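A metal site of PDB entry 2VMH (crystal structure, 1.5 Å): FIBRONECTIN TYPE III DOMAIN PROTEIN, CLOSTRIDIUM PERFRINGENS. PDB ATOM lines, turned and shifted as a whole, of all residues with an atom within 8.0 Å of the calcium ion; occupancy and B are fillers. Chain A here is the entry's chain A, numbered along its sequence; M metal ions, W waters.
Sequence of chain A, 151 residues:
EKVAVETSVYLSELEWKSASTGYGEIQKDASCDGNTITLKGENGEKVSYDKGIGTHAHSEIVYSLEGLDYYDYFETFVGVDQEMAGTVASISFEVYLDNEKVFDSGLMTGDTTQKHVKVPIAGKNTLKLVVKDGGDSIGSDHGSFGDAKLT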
ATOM      1  N   HIS A  56     -16.174  24.895   0.195  1.00  0.00           N
ATOM      2  CA  HIS A  56     -16.821  24.390   1.393  1.00  0.00           C
ATOM      3  C   HIS A  56     -15.750  23.999   2.399  1.00  0.00           C
ATOM      4  O   HIS A  56     -14.833  23.270   2.022  1.00  0.00           O
ATOM      5  CB  HIS A  56     -17.674  23.148   1.017  1.00  0.00           C
ATOM      6  CG  HIS A  56     -18.672  22.722   2.053  1.00  0.00           C
ATOM      7  ND1 HIS A  56     -18.310  22.268   3.309  1.00  0.00           N
ATOM      8  CD2 HIS A  56     -20.020  22.668   2.017  1.00  0.00           C
ATOM      9  CE1 HIS A  56     -19.403  21.927   3.993  1.00  0.00           C
ATOM     10  NE2 HIS A  56     -20.461  22.200   3.249  1.00  0.00           N
ATOM     11  N   ALA A  57     -15.865  24.434   3.653  1.00  0.00           N
ATOM     12  CA  ALA A  57     -14.878  24.034   4.647  1.00  0.00           C
ATOM     13  C   ALA A  57     -14.888  22.490   4.783  1.00  0.00           C
ATOM     14  O   ALA A  57     -15.946  21.877   4.579  1.00  0.00           O
ATOM     15  CB  ALA A  57     -15.172  24.631   6.044  1.00  0.00           C
ATOM     16  N   VAL A  88     -26.619  26.996  10.283  1.00  0.00           N
ATOM     17  CA  VAL A  88     -25.514  26.867  11.257  1.00  0.00           C
ATOM     18  C   VAL A  88     -24.153  27.189  10.647  1.00  0.00           C
ATOM     19  O   VAL A  88     -23.127  27.049  11.327  1.00  0.00           O
ATOM     20  CB  VAL A  88     -25.528  25.417  11.864  1.00  0.00           C
ATOM     21  CG1 VAL A  88     -25.078  24.391  10.862  1.00  0.00           C
ATOM     22  CG2 VAL A  88     -24.799  25.345  13.197  1.00  0.00           C
ATOM     23  N   ALA A  89     -24.131  27.646   9.394  1.00  0.00           N
ATOM     24  CA  ALA A  89     -22.851  28.008   8.721  1.00  0.00           C
ATOM     25  C   ALA A  89     -21.944  28.777   9.674  1.00  0.00           C
ATOM     26  O   ALA A  89     -22.360  29.801  10.261  1.00  0.00           O
ATOM     27  CB  ALA A  89     -23.151  28.906   7.472  1.00  0.00           C
ATOM     28  N   SER A  90     -20.695  28.368   9.715  1.00  0.00           N
ATOM     29  CA  SER A  90     -19.705  29.028  10.568  1.00  0.00           C
ATOM     30  C   SER A  90     -18.321  28.652  10.059  1.00  0.00           C
ATOM     31  O   SER A  90     -17.890  27.489  10.096  1.00  0.00           O
ATOM     32  CB  SER A  90     -19.861  28.542  12.032  1.00  0.00           C
ATOM     33  OG  SER A  90     -19.843  27.146  12.137  1.00  0.00           O
ATOM     34  N   ILE A  91     -17.602  29.650   9.606  1.00  0.00           N
ATOM     35  CA  ILE A  91     -16.334  29.447   8.933  1.00  0.00           C
ATOM     36  C   ILE A  91     -15.342  30.571   9.217  1.00  0.00           C
ATOM     37  O   ILE A  91     -15.706  31.593   9.753  1.00  0.00           O
ATOM     38  CB  ILE A  91     -16.564  29.372   7.381  1.00  0.00           C
ATOM     39  CG1 ILE A  91     -17.091  30.694   6.814  1.00  0.00           C
ATOM     40  CG2 ILE A  91     -17.398  28.145   7.027  1.00  0.00           C
ATOM     41  CD1 ILE A  91     -17.439  30.606   5.311  1.00  0.00           C
ATOM     42  N   SER A  92     -14.115  30.371   8.806  1.00  0.00           N
ATOM     43  CA  SER A  92     -13.174  31.508   8.733  1.00  0.00           C
ATOM     44  C   SER A  92     -12.395  31.331   7.456  1.00  0.00           C
ATOM     45  O   SER A  92     -12.262  30.195   6.901  1.00  0.00           O
ATOM     46  CB  SER A  92     -12.204  31.606   9.934  1.00  0.00           C
ATOM     47  OG  SER A  92     -11.349  30.475   9.997  1.00  0.00           O
ATOM     48  N   LEU A 107     -14.110  34.370  12.801  1.00  0.00           N
ATOM     49  CA  LEU A 107     -15.365  33.653  12.620  1.00  0.00           C
ATOM     50  C   LEU A 107     -16.334  34.477  11.826  1.00  0.00           C
ATOM     51  O   LEU A 107     -16.590  35.646  12.145  1.00  0.00           O
ATOM     52  CB  LEU A 107     -15.940  33.336  13.983  1.00  0.00           C
ATOM     53  CG  LEU A 107     -17.292  32.608  14.000  1.00  0.00           C
ATOM     54  CD1 LEU A 107     -17.248  31.183  13.377  1.00  0.00           C
ATOM     55  CD2 LEU A 107     -17.853  32.525  15.467  1.00  0.00           C
ATOM     56  N   MET A 108     -16.983  33.815  10.848  1.00  0.00           N
ATOM     57  CA  MET A 108     -18.082  34.376  10.090  1.00  0.00           C
ATOM     58  C   MET A 108     -19.225  33.346  10.119  1.00  0.00           C
ATOM     59  O   MET A 108     -19.019  32.177   9.806  1.00  0.00           O
ATOM     60  CB  MET A 108     -17.667  34.684   8.639  1.00  0.00           C
ATOM     61  CG  MET A 108     -16.437  35.597   8.547  1.00  0.00           C
ATOM     62  SD  MET A 108     -16.115  36.130   6.869  1.00  0.00           S
ATOM     63  CE  MET A 108     -17.442  37.353   6.627  1.00  0.00           C
ATOM     64  N   THR A 109     -20.397  33.844  10.489  1.00  0.00           N
ATOM     65  CA  THR A 109     -21.591  33.055  10.439  1.00  0.00           C
ATOM     66  C   THR A 109     -22.489  33.579   9.274  1.00  0.00           C
ATOM     67  O   THR A 109     -22.098  34.469   8.512  1.00  0.00           O
ATOM     68  CB  THR A 109     -22.313  33.032  11.767  1.00  0.00           C
ATOM     69  OG1 THR A 109     -22.561  34.380  12.160  1.00  0.00           O
ATOM     70  CG2 THR A 109     -21.444  32.392  12.805  1.00  0.00           C
ATOM     71  N   LYS A 132     -11.809  27.410   6.801  1.00  0.00           N
ATOM     72  CA  LYS A 132     -11.874  26.540   7.980  1.00  0.00           C
ATOM     73  C   LYS A 132     -13.307  26.474   8.500  1.00  0.00           C
ATOM     74  O   LYS A 132     -14.150  27.307   8.150  1.00  0.00           O
ATOM     75  CB  LYS A 132     -10.962  27.072   9.090  1.00  0.00           C
ATOM     76  CG  LYS A 132      -9.468  26.985   8.739  1.00  0.00           C
ATOM     77  CD  LYS A 132      -8.622  27.635   9.833  1.00  0.00           C
ATOM     78  CE  LYS A 132      -7.190  27.171   9.822  1.00  0.00           C
ATOM     79  NZ  LYS A 132      -6.381  27.865  10.921  1.00  0.00           N
ATOM     80  N   ASP A 133     -13.545  25.512   9.397  1.00  0.00           N
ATOM     81  CA  ASP A 133     -14.907  25.136   9.740  1.00  0.00           C
ATOM     82  C   ASP A 133     -15.502  25.834  10.982  1.00  0.00           C
ATOM     83  O   ASP A 133     -16.516  25.389  11.508  1.00  0.00           O
ATOM     84  CB  ASP A 133     -14.943  23.612   9.978  1.00  0.00           C
ATOM     85  CG  ASP A 133     -14.281  23.185  11.272  1.00  0.00           C
ATOM     86  OD1 ASP A 133     -13.692  24.029  12.025  1.00  0.00           O
ATOM     87  OD2 ASP A 133     -14.319  21.938  11.516  1.00  0.00           O
ATOM     88  N   GLY A 134     -14.900  26.912  11.440  1.00  0.00           N
ATOM     89  CA  GLY A 134     -15.457  27.704  12.550  1.00  0.00           C
ATOM     90  C   GLY A 134     -15.361  27.032  13.897  1.00  0.00           C
ATOM     91  O   GLY A 134     -15.897  27.566  14.875  1.00  0.00           O
ATOM     92  N   GLY A 135     -14.690  25.881  13.962  1.00  0.00           N
ATOM     93  CA  GLY A 135     -14.443  25.157  15.228  1.00  0.00           C
ATOM     94  C   GLY A 135     -15.596  24.291  15.729  1.00  0.00           C
ATOM     95  O   GLY A 135     -15.538  23.754  16.872  1.00  0.00           O
ATOM     96  N   ASP A 136     -16.616  24.117  14.882  1.00  0.00           N
ATOM     97  CA  ASP A 136     -17.725  23.243  15.224  1.00  0.00           C
ATOM     98  C   ASP A 136     -17.808  21.944  14.394  1.00  0.00           C
ATOM     99  O   ASP A 136     -17.348  20.857  14.850  1.00  0.00           O
ATOM    100  CB  ASP A 136     -19.062  24.000  15.353  1.00  0.00           C
ATOM    101  CG  ASP A 136     -19.322  24.964  14.234  1.00  0.00           C
ATOM    102  OD1 ASP A 136     -18.734  24.745  13.170  1.00  0.00           O
ATOM    103  OD2 ASP A 136     -20.089  25.945  14.481  1.00  0.00           O
ATOM    104  N   SER A 137     -18.470  22.019  13.257  1.00  0.00           N
ATOM    105  CA  SER A 137     -18.482  20.992  12.222  1.00  0.00           C
ATOM    106  C   SER A 137     -18.504  21.722  10.884  1.00  0.00           C
ATOM    107  O   SER A 137     -18.700  22.938  10.864  1.00  0.00           O
ATOM    108  CB  SER A 137     -19.748  20.134  12.332  1.00  0.00           C
ATOM    109  OG  SER A 137     -20.875  20.757  11.723  1.00  0.00           O
ATOM    110  N   ILE A 138     -18.355  20.985   9.808  1.00  0.00           N
ATOM    111  CA  ILE A 138     -18.440  21.629   8.476  1.00  0.00           C
ATOM    112  C   ILE A 138     -19.869  21.843   7.982  1.00  0.00           C
ATOM    113  O   ILE A 138     -20.085  22.304   6.839  1.00  0.00           O
ATOM    114  CB  ILE A 138     -17.624  20.844   7.381  1.00  0.00           C
ATOM    115  CG1 ILE A 138     -18.210  19.440   7.102  1.00  0.00           C
ATOM    116  CG2 ILE A 138     -16.107  20.746   7.771  1.00  0.00           C
ATOM    117  CD1 ILE A 138     -17.576  18.771   5.861  1.00  0.00           C
ATOM    118  N   GLY A 139     -20.869  21.592   8.837  1.00  0.00           N
ATOM    119  CA  GLY A 139     -22.262  21.695   8.412  1.00  0.00           C
ATOM    120  C   GLY A 139     -22.584  23.096   7.904  1.00  0.00           C
ATOM    121  O   GLY A 139     -22.386  24.057   8.636  1.00  0.00           O
ATOM    122  N   SER A 140     -23.047  23.179   6.658  1.00  0.00           N
ATOM    123  CA  SER A 140     -23.492  24.446   6.052  1.00  0.00           C
ATOM    124  C   SER A 140     -22.340  25.413   5.740  1.00  0.00           C
ATOM    125  O   SER A 140     -22.588  26.582   5.393  1.00  0.00           O
ATOM    126  CB  SER A 140     -24.544  25.136   6.900  1.00  0.00           C
ATOM    127  OG  SER A 140     -25.671  24.337   6.964  1.00  0.00           O
ATOM    128  N   ASP A 141     -21.107  24.909   5.812  1.00  0.00           N
ATOM    129  CA  ASP A 141     -19.902  25.795   5.693  1.00  0.00           C
ATOM    130  C   ASP A 141     -19.550  26.140   4.234  1.00  0.00           C
ATOM    131  O   ASP A 141     -18.456  25.825   3.754  1.00  0.00           O
ATOM    132  CB  ASP A 141     -18.741  25.164   6.434  1.00  0.00           C
ATOM    133  CG  ASP A 141     -18.836  25.320   7.965  1.00  0.00           C
ATOM    134  OD1 ASP A 141     -19.847  25.933   8.498  1.00  0.00           O
ATOM    135  OD2 ASP A 141     -17.843  24.843   8.603  1.00  0.00           O
ATOM    136  N   HIS A 142     -20.516  26.713   3.526  1.00  0.00           N
ATOM    137  CA  HIS A 142     -20.319  27.121   2.169  1.00  0.00           C
ATOM    138  C   HIS A 142     -19.665  28.507   2.187  1.00  0.00           C
ATOM    139  O   HIS A 142     -20.271  29.472   2.657  1.00  0.00           O
ATOM    140  CB  HIS A 142     -21.655  27.283   1.449  1.00  0.00           C
ATOM    141  CG  HIS A 142     -22.473  26.022   1.374  1.00  0.00           C
ATOM    142  ND1 HIS A 142     -23.403  25.820   0.380  1.00  0.00           N
ATOM    143  CD2 HIS A 142     -22.521  24.923   2.182  1.00  0.00           C
ATOM    144  CE1 HIS A 142     -24.012  24.650   0.585  1.00  0.00           C
ATOM    145  NE2 HIS A 142     -23.490  24.080   1.668  1.00  0.00           N
HETATM  146 CA    CA M   1     -18.798  25.324  10.819  1.00  0.00          CA
HETATM  147  O   HOH W   1     -21.236  24.857  11.009  1.00  0.00           O
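The side-chain carboxylate (OD1) of Asp 133 sits at hydrogen-bond distance from the backbone NH (N) of Gly 135 (2.9 Å). The side-chain hydroxyl of Ser 137 sits at hydrogen-bond distance from the backbone NH of Gly 139. The backbone carbonyl oxygen of Ser 90 sits close to the backbone NH of Gly 134, 3.3 Å away. The backbone carbonyl oxygen (O) of Val 88 sits close to the side-chain hydroxyl (OG) of Ser 90 (3.4 Å). The backbone NH (N) of Ala 57 sits at hydrogen-bond distance from the backbone carbonyl oxygen (O) of Asp 141, at 2.9 Å.
Of the 21 residues printed, 5 come within 4 Å of the calcium ion.
The calcium ion is bound by the backbone carbonyl oxygen (O) of Asp 133 (2.4 Å). O of Ser 137 is bound to the calcium ion (2.4 Å). The side-chain carboxylate (OD1) of Asp 136 binds the calcium ion, 2.4 Å away. O of Ser 90 binds the calcium ion (2.5 Å). OD2 of Asp 141 binds the calcium ion (2.5 Å). The side-chain hydroxyl (OG) of Ser 90 binds the calcium ion (2.5 Å). The calcium ion is bound by water W1, 2.5 Å away. OD1 of Asp 141 binds the calcium ion, at 2.6 Å.
Water W1 lies within hydrogen-bond range of O of Gly 139 (2.8 Å) and O of Val 88 (2.9 Å).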
